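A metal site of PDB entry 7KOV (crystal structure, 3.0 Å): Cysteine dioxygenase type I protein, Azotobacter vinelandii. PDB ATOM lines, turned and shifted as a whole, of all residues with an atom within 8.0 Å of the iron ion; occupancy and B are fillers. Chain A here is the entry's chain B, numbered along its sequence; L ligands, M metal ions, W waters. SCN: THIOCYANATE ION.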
ATOM      1  N   TYR A  61      24.027 -30.203  -7.185  1.00  0.00           N
ATOM      2  CA  TYR A  61      24.657 -30.991  -8.287  1.00  0.00           C
ATOM      3  C   TYR A  61      26.160 -30.697  -8.292  1.00  0.00           C
ATOM      4  O   TYR A  61      26.551 -29.532  -8.032  1.00  0.00           O
ATOM      5  CB  TYR A  61      23.997 -30.667  -9.629  1.00  0.00           C
ATOM      6  CG  TYR A  61      24.341 -29.330 -10.236  1.00  0.00           C
ATOM      7  CD1 TYR A  61      25.298 -29.217 -11.232  1.00  0.00           C
ATOM      8  CD2 TYR A  61      23.704 -28.171  -9.825  1.00  0.00           C
ATOM      9  CE1 TYR A  61      25.621 -27.994 -11.804  1.00  0.00           C
ATOM     10  CE2 TYR A  61      24.019 -26.941 -10.375  1.00  0.00           C
ATOM     11  CZ  TYR A  61      24.976 -26.851 -11.376  1.00  0.00           C
ATOM     12  OH  TYR A  61      25.289 -25.640 -11.916  1.00  0.00           O
ATOM     13  N   GLN A  63      30.088 -30.647  -9.984  1.00  0.00           N
ATOM     14  CA  GLN A  63      30.832 -30.378 -11.236  1.00  0.00           C
ATOM     15  C   GLN A  63      32.301 -30.760 -11.021  1.00  0.00           C
ATOM     16  O   GLN A  63      33.041 -29.953 -10.420  1.00  0.00           O
ATOM     17  CB  GLN A  63      30.739 -28.896 -11.599  1.00  0.00           C
ATOM     18  CG  GLN A  63      29.326 -28.420 -11.862  1.00  0.00           C
ATOM     19  CD  GLN A  63      29.236 -26.909 -11.845  1.00  0.00           C
ATOM     20  OE1 GLN A  63      29.665 -26.263 -10.891  1.00  0.00           O
ATOM     21  NE2 GLN A  63      28.664 -26.351 -12.894  1.00  0.00           N
ATOM     22  N   PHE A  79      29.528 -33.771 -14.792  1.00  0.00           N
ATOM     23  CA  PHE A  79      28.372 -33.229 -14.038  1.00  0.00           C
ATOM     24  C   PHE A  79      27.583 -34.407 -13.465  1.00  0.00           C
ATOM     25  O   PHE A  79      27.252 -35.326 -14.234  1.00  0.00           O
ATOM     26  CB  PHE A  79      27.468 -32.381 -14.945  1.00  0.00           C
ATOM     27  CG  PHE A  79      27.955 -30.984 -15.244  1.00  0.00           C
ATOM     28  CD1 PHE A  79      27.167 -29.889 -14.955  1.00  0.00           C
ATOM     29  CD2 PHE A  79      29.189 -30.766 -15.846  1.00  0.00           C
ATOM     30  CE1 PHE A  79      27.598 -28.595 -15.240  1.00  0.00           C
ATOM     31  CE2 PHE A  79      29.623 -29.478 -16.123  1.00  0.00           C
ATOM     32  CZ  PHE A  79      28.826 -28.399 -15.818  1.00  0.00           C
ATOM     33  N   TRP A  81      24.181 -35.311 -11.108  1.00  0.00           N
ATOM     34  CA  TRP A  81      22.888 -34.925 -10.476  1.00  0.00           C
ATOM     35  C   TRP A  81      22.391 -36.065  -9.581  1.00  0.00           C
ATOM     36  O   TRP A  81      22.289 -37.208 -10.088  1.00  0.00           O
ATOM     37  CB  TRP A  81      21.836 -34.568 -11.533  1.00  0.00           C
ATOM     38  CG  TRP A  81      22.138 -33.324 -12.307  1.00  0.00           C
ATOM     39  CD1 TRP A  81      21.699 -32.062 -12.021  1.00  0.00           C
ATOM     40  CD2 TRP A  81      22.915 -33.220 -13.505  1.00  0.00           C
ATOM     41  NE1 TRP A  81      22.167 -31.175 -12.964  1.00  0.00           N
ATOM     42  CE2 TRP A  81      22.911 -31.861 -13.889  1.00  0.00           C
ATOM     43  CE3 TRP A  81      23.606 -34.137 -14.294  1.00  0.00           C
ATOM     44  CZ2 TRP A  81      23.581 -31.403 -15.018  1.00  0.00           C
ATOM     45  CZ3 TRP A  81      24.265 -33.689 -15.414  1.00  0.00           C
ATOM     46  CH2 TRP A  81      24.250 -32.335 -15.773  1.00  0.00           C
ATOM     47  N   THR A  87      20.302 -28.019 -12.548  1.00  0.00           N
ATOM     48  CA  THR A  87      21.026 -26.741 -12.754  1.00  0.00           C
ATOM     49  C   THR A  87      20.000 -25.615 -12.762  1.00  0.00           C
ATOM     50  O   THR A  87      18.825 -25.851 -13.000  1.00  0.00           O
ATOM     51  CB  THR A  87      21.797 -26.699 -14.079  1.00  0.00           C
ATOM     52  OG1 THR A  87      20.850 -26.582 -15.139  1.00  0.00           O
ATOM     53  CG2 THR A  87      22.697 -27.900 -14.304  1.00  0.00           C
ATOM     54  N   PRO A  88      20.411 -24.352 -12.509  1.00  0.00           N
ATOM     55  CA  PRO A  88      19.542 -23.218 -12.785  1.00  0.00           C
ATOM     56  C   PRO A  88      19.540 -23.021 -14.308  1.00  0.00           C
ATOM     57  O   PRO A  88      20.369 -23.616 -14.974  1.00  0.00           O
ATOM     58  CB  PRO A  88      20.226 -22.059 -12.055  1.00  0.00           C
ATOM     59  CG  PRO A  88      21.697 -22.428 -12.081  1.00  0.00           C
ATOM     60  CD  PRO A  88      21.718 -23.949 -11.965  1.00  0.00           C
ATOM     61  N   VAL A  89      18.606 -22.209 -14.824  1.00  0.00           N
ATOM     62  CA  VAL A  89      18.665 -21.727 -16.228  1.00  0.00           C
ATOM     63  C   VAL A  89      19.952 -20.906 -16.347  1.00  0.00           C
ATOM     64  O   VAL A  89      20.147 -20.030 -15.490  1.00  0.00           O
ATOM     65  CB  VAL A  89      17.419 -20.913 -16.629  1.00  0.00           C
ATOM     66  CG1 VAL A  89      17.491 -20.464 -18.091  1.00  0.00           C
ATOM     67  CG2 VAL A  89      16.128 -21.662 -16.345  1.00  0.00           C
ATOM     68  N   HIS A  90      20.812 -21.212 -17.320  1.00  0.00           N
ATOM     69  CA  HIS A  90      22.164 -20.605 -17.460  1.00  0.00           C
ATOM     70  C   HIS A  90      22.583 -20.582 -18.940  1.00  0.00           C
ATOM     71  O   HIS A  90      22.051 -21.404 -19.712  1.00  0.00           O
ATOM     72  CB  HIS A  90      23.179 -21.361 -16.594  1.00  0.00           C
ATOM     73  CG  HIS A  90      23.401 -22.770 -17.035  1.00  0.00           C
ATOM     74  ND1 HIS A  90      22.692 -23.834 -16.502  1.00  0.00           N
ATOM     75  CD2 HIS A  90      24.231 -23.303 -17.956  1.00  0.00           C
ATOM     76  CE1 HIS A  90      23.081 -24.949 -17.076  1.00  0.00           C
ATOM     77  NE2 HIS A  90      24.025 -24.649 -17.971  1.00  0.00           N
ATOM     78  N   ASP A  91      23.499 -19.667 -19.289  1.00  0.00           N
ATOM     79  CA  ASP A  91      24.193 -19.633 -20.595  1.00  0.00           C
ATOM     80  C   ASP A  91      25.647 -20.062 -20.374  1.00  0.00           C
ATOM     81  O   ASP A  91      25.982 -20.357 -19.209  1.00  0.00           O
ATOM     82  CB  ASP A  91      24.047 -18.267 -21.286  1.00  0.00           C
ATOM     83  CG  ASP A  91      24.646 -17.089 -20.526  1.00  0.00           C
ATOM     84  OD1 ASP A  91      25.179 -17.294 -19.419  1.00  0.00           O
ATOM     85  OD2 ASP A  91      24.572 -15.971 -21.070  1.00  0.00           O
ATOM     86  N   HIS A  92      26.459 -20.089 -21.436  1.00  0.00           N
ATOM     87  CA  HIS A  92      27.842 -20.626 -21.438  1.00  0.00           C
ATOM     88  C   HIS A  92      28.826 -19.596 -22.007  1.00  0.00           C
ATOM     89  O   HIS A  92      29.948 -19.480 -21.464  1.00  0.00           O
ATOM     90  CB  HIS A  92      27.875 -21.950 -22.213  1.00  0.00           C
ATOM     91  CG  HIS A  92      26.827 -22.897 -21.756  1.00  0.00           C
ATOM     92  ND1 HIS A  92      25.569 -22.941 -22.343  1.00  0.00           N
ATOM     93  CD2 HIS A  92      26.804 -23.794 -20.752  1.00  0.00           C
ATOM     94  CE1 HIS A  92      24.836 -23.838 -21.734  1.00  0.00           C
ATOM     95  NE2 HIS A  92      25.561 -24.379 -20.747  1.00  0.00           N
ATOM     96  N   GLY A  96      29.698 -25.576 -26.348  1.00  0.00           N
ATOM     97  CA  GLY A  96      29.599 -26.692 -25.390  1.00  0.00           C
ATOM     98  C   GLY A  96      29.099 -27.952 -26.062  1.00  0.00           C
ATOM     99  O   GLY A  96      28.337 -27.842 -27.041  1.00  0.00           O
ATOM    100  N   ILE A  98      27.401 -31.627 -24.514  1.00  0.00           N
ATOM    101  CA  ILE A  98      26.944 -32.482 -23.376  1.00  0.00           C
ATOM    102  C   ILE A  98      26.792 -33.920 -23.880  1.00  0.00           C
ATOM    103  O   ILE A  98      25.892 -34.164 -24.703  1.00  0.00           O
ATOM    104  CB  ILE A  98      25.642 -31.949 -22.729  1.00  0.00           C
ATOM    105  CG1 ILE A  98      24.979 -33.010 -21.850  1.00  0.00           C
ATOM    106  CG2 ILE A  98      24.678 -31.391 -23.771  1.00  0.00           C
ATOM    107  CD1 ILE A  98      23.932 -32.467 -20.904  1.00  0.00           C
ATOM    108  N   VAL A 134      25.637 -26.721 -27.352  1.00  0.00           N
ATOM    109  CA  VAL A 134      25.169 -25.349 -26.982  1.00  0.00           C
ATOM    110  C   VAL A 134      26.264 -24.356 -27.391  1.00  0.00           C
ATOM    111  O   VAL A 134      27.446 -24.742 -27.392  1.00  0.00           O
ATOM    112  CB  VAL A 134      24.836 -25.238 -25.488  1.00  0.00           C
ATOM    113  CG1 VAL A 134      23.757 -26.233 -25.072  1.00  0.00           C
ATOM    114  CG2 VAL A 134      26.074 -25.400 -24.610  1.00  0.00           C
ATOM    115  N   ASP A 140      22.145 -20.850 -26.541  1.00  0.00           N
ATOM    116  CA  ASP A 140      23.154 -20.844 -25.440  1.00  0.00           C
ATOM    117  C   ASP A 140      22.495 -21.073 -24.077  1.00  0.00           C
ATOM    118  O   ASP A 140      23.219 -21.481 -23.154  1.00  0.00           O
ATOM    119  CB  ASP A 140      23.915 -19.517 -25.420  1.00  0.00           C
ATOM    120  CG  ASP A 140      25.293 -19.606 -24.780  1.00  0.00           C
ATOM    121  OD1 ASP A 140      25.797 -20.741 -24.626  1.00  0.00           O
ATOM    122  OD2 ASP A 140      25.845 -18.539 -24.439  1.00  0.00           O
ATOM    123  N   ILE A 141      21.188 -20.805 -23.946  1.00  0.00           N
ATOM    124  CA  ILE A 141      20.459 -20.869 -22.639  1.00  0.00           C
ATOM    125  C   ILE A 141      19.707 -22.203 -22.562  1.00  0.00           C
ATOM    126  O   ILE A 141      19.024 -22.539 -23.556  1.00  0.00           O
ATOM    127  CB  ILE A 141      19.499 -19.674 -22.467  1.00  0.00           C
ATOM    128  CG1 ILE A 141      20.173 -18.346 -22.841  1.00  0.00           C
ATOM    129  CG2 ILE A 141      18.928 -19.628 -21.054  1.00  0.00           C
ATOM    130  CD1 ILE A 141      19.319 -17.125 -22.615  1.00  0.00           C
ATOM    131  N   HIS A 142      19.843 -22.918 -21.435  1.00  0.00           N
ATOM    132  CA  HIS A 142      19.147 -24.196 -21.145  1.00  0.00           C
ATOM    133  C   HIS A 142      19.098 -24.468 -19.640  1.00  0.00           C
ATOM    134  O   HIS A 142      19.650 -23.663 -18.862  1.00  0.00           O
ATOM    135  CB  HIS A 142      19.779 -25.369 -21.911  1.00  0.00           C
ATOM    136  CG  HIS A 142      21.124 -25.817 -21.417  1.00  0.00           C
ATOM    137  ND1 HIS A 142      21.821 -26.838 -22.054  1.00  0.00           N
ATOM    138  CD2 HIS A 142      21.905 -25.405 -20.394  1.00  0.00           C
ATOM    139  CE1 HIS A 142      22.964 -27.033 -21.425  1.00  0.00           C
ATOM    140  NE2 HIS A 142      23.046 -26.166 -20.406  1.00  0.00           N
ATOM    141  N   ARG A 143      18.449 -25.570 -19.263  1.00  0.00           N
ATOM    142  CA  ARG A 143      18.369 -26.129 -17.887  1.00  0.00           C
ATOM    143  C   ARG A 143      18.457 -27.651 -17.979  1.00  0.00           C
ATOM    144  O   ARG A 143      17.545 -28.257 -18.561  1.00  0.00           O
ATOM    145  CB  ARG A 143      17.062 -25.696 -17.226  1.00  0.00           C
ATOM    146  CG  ARG A 143      16.858 -26.234 -15.821  1.00  0.00           C
ATOM    147  CD  ARG A 143      15.579 -25.700 -15.179  1.00  0.00           C
ATOM    148  NE  ARG A 143      14.403 -26.463 -15.551  1.00  0.00           N
ATOM    149  CZ  ARG A 143      13.954 -27.554 -14.925  1.00  0.00           C
ATOM    150  NH1 ARG A 143      14.586 -28.040 -13.864  1.00  0.00           N
ATOM    151  NH2 ARG A 143      12.867 -28.167 -15.364  1.00  0.00           N
ATOM    152  N   VAL A 144      19.526 -28.244 -17.422  1.00  0.00           N
ATOM    153  CA  VAL A 144      19.746 -29.728 -17.367  1.00  0.00           C
ATOM    154  C   VAL A 144      19.311 -30.220 -15.983  1.00  0.00           C
ATOM    155  O   VAL A 144      19.696 -29.592 -14.989  1.00  0.00           O
ATOM    156  CB  VAL A 144      21.214 -30.072 -17.650  1.00  0.00           C
ATOM    157  CG1 VAL A 144      21.417 -31.563 -17.874  1.00  0.00           C
ATOM    158  CG2 VAL A 144      21.754 -29.277 -18.837  1.00  0.00           C
ATOM    159  N   HIS A 157      30.522 -33.095 -19.955  1.00  0.00           N
ATOM    160  CA  HIS A 157      30.403 -31.792 -20.666  1.00  0.00           C
ATOM    161  C   HIS A 157      31.789 -31.369 -21.152  1.00  0.00           C
ATOM    162  O   HIS A 157      32.757 -31.494 -20.370  1.00  0.00           O
ATOM    163  CB  HIS A 157      29.764 -30.732 -19.764  1.00  0.00           C
ATOM    164  CG  HIS A 157      28.385 -31.065 -19.301  1.00  0.00           C
ATOM    165  ND1 HIS A 157      27.440 -30.092 -19.048  1.00  0.00           N
ATOM    166  CD2 HIS A 157      27.790 -32.243 -19.029  1.00  0.00           C
ATOM    167  CE1 HIS A 157      26.314 -30.657 -18.654  1.00  0.00           C
ATOM    168  NE2 HIS A 157      26.504 -31.978 -18.629  1.00  0.00           N
ATOM    169  N   TYR A 159      33.637 -27.931 -23.085  1.00  0.00           N
ATOM    170  CA  TYR A 159      33.433 -26.478 -23.370  1.00  0.00           C
ATOM    171  C   TYR A 159      34.677 -25.903 -24.057  1.00  0.00           C
ATOM    172  O   TYR A 159      35.779 -26.476 -23.892  1.00  0.00           O
ATOM    173  CB  TYR A 159      33.137 -25.718 -22.078  1.00  0.00           C
ATOM    174  CG  TYR A 159      31.944 -26.225 -21.311  1.00  0.00           C
ATOM    175  CD1 TYR A 159      30.668 -25.765 -21.605  1.00  0.00           C
ATOM    176  CD2 TYR A 159      32.089 -27.130 -20.273  1.00  0.00           C
ATOM    177  CE1 TYR A 159      29.564 -26.209 -20.895  1.00  0.00           C
ATOM    178  CE2 TYR A 159      30.992 -27.573 -19.552  1.00  0.00           C
ATOM    179  CZ  TYR A 159      29.722 -27.109 -19.858  1.00  0.00           C
ATOM    180  OH  TYR A 159      28.642 -27.535 -19.141  1.00  0.00           O
ATOM    181  N   ILE A 163      35.637 -23.776 -18.143  1.00  0.00           N
ATOM    182  CA  ILE A 163      34.203 -23.406 -17.902  1.00  0.00           C
ATOM    183  C   ILE A 163      33.997 -22.905 -16.465  1.00  0.00           C
ATOM    184  O   ILE A 163      33.137 -22.028 -16.276  1.00  0.00           O
ATOM    185  CB  ILE A 163      33.268 -24.578 -18.232  1.00  0.00           C
ATOM    186  CG1 ILE A 163      31.797 -24.149 -18.263  1.00  0.00           C
ATOM    187  CG2 ILE A 163      33.489 -25.743 -17.269  1.00  0.00           C
ATOM    188  CD1 ILE A 163      31.512 -23.044 -19.252  1.00  0.00           C
ATOM    189  N   ARG A 168      29.792 -15.897 -16.692  1.00  0.00           N
ATOM    190  CA  ARG A 168      28.530 -16.088 -17.449  1.00  0.00           C
ATOM    191  C   ARG A 168      27.373 -15.716 -16.515  1.00  0.00           C
ATOM    192  O   ARG A 168      27.623 -14.949 -15.564  1.00  0.00           O
ATOM    193  CB  ARG A 168      28.463 -17.504 -18.029  1.00  0.00           C
ATOM    194  CG  ARG A 168      28.603 -18.638 -17.016  1.00  0.00           C
ATOM    195  CD  ARG A 168      29.057 -19.916 -17.703  1.00  0.00           C
ATOM    196  NE  ARG A 168      29.274 -21.034 -16.794  1.00  0.00           N
ATOM    197  CZ  ARG A 168      28.565 -22.156 -16.759  1.00  0.00           C
ATOM    198  NH1 ARG A 168      27.545 -22.352 -17.584  1.00  0.00           N
ATOM    199  NH2 ARG A 168      28.880 -23.095 -15.883  1.00  0.00           N
ATOM    200  N   PHE A 180      27.372 -15.317 -12.880  1.00  0.00           N
ATOM    201  CA  PHE A 180      27.532 -16.763 -12.549  1.00  0.00           C
ATOM    202  C   PHE A 180      28.956 -17.212 -12.877  1.00  0.00           C
ATOM    203  O   PHE A 180      29.365 -17.119 -14.059  1.00  0.00           O
ATOM    204  CB  PHE A 180      26.487 -17.579 -13.312  1.00  0.00           C
ATOM    205  CG  PHE A 180      26.479 -19.066 -13.026  1.00  0.00           C
ATOM    206  CD1 PHE A 180      26.492 -19.539 -11.731  1.00  0.00           C
ATOM    207  CD2 PHE A 180      26.426 -19.982 -14.067  1.00  0.00           C
ATOM    208  CE1 PHE A 180      26.458 -20.898 -11.466  1.00  0.00           C
ATOM    209  CE2 PHE A 180      26.399 -21.344 -13.808  1.00  0.00           C
ATOM    210  CZ  PHE A 180      26.413 -21.794 -12.507  1.00  0.00           C
HETATM  211  S   SCN L   1      27.347 -28.576 -22.840  1.00  0.00           S
HETATM  212  C   SCN L   1      26.629 -27.847 -21.664  1.00  0.00           C
HETATM  213  N   SCN L   1      26.097 -27.304 -20.790  1.00  0.00           N
HETATM  214 FE    FE M   1      24.995 -26.009 -19.406  1.00  0.00          FE
HETATM  215  O   HOH W   1      25.215 -27.698 -18.005  1.00  0.00           O
HETATM  216  O   HOH W   2      26.850 -25.760 -17.744  1.00  0.00           O
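The backbone carbonyl oxygen (O) of Asp 140 sits at hydrogen-bond distance from a ring nitrogen (ND1) of His 92, at 2.9 Å. A ring nitrogen (ND1) of His 90 sits at hydrogen-bond distance from the backbone carbonyl oxygen of Pro 88 (2.8 Å). The side-chain hydroxyl of Tyr 159 is in hydrogen-bond range of a ring nitrogen (ND1) of His 157 (2.8 Å).
NE2 of His 92 is bound to the iron ion (2.2 Å). The iron ion is bound by a nitrogen (N) of the ligand (2.2 Å). NE2 of His 142 binds the iron ion, 2.2 Å away. A ring nitrogen (NE2) of His 90 binds the iron ion (2.2 Å). The iron ion is bound by water W1, at 2.2 Å. The iron ion is bound by water W2, 2.5 Å away. The iron ion has six donor atoms within binding distance.
Residues that only touch the iron ion: Tyr 159 (3.96 Å).
Water W2 bridges the side-chain hydroxyl (OH) of Tyr 159 (2.9 Å) and the guanidinium group (NH1) of Arg 168 (3.5 Å).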
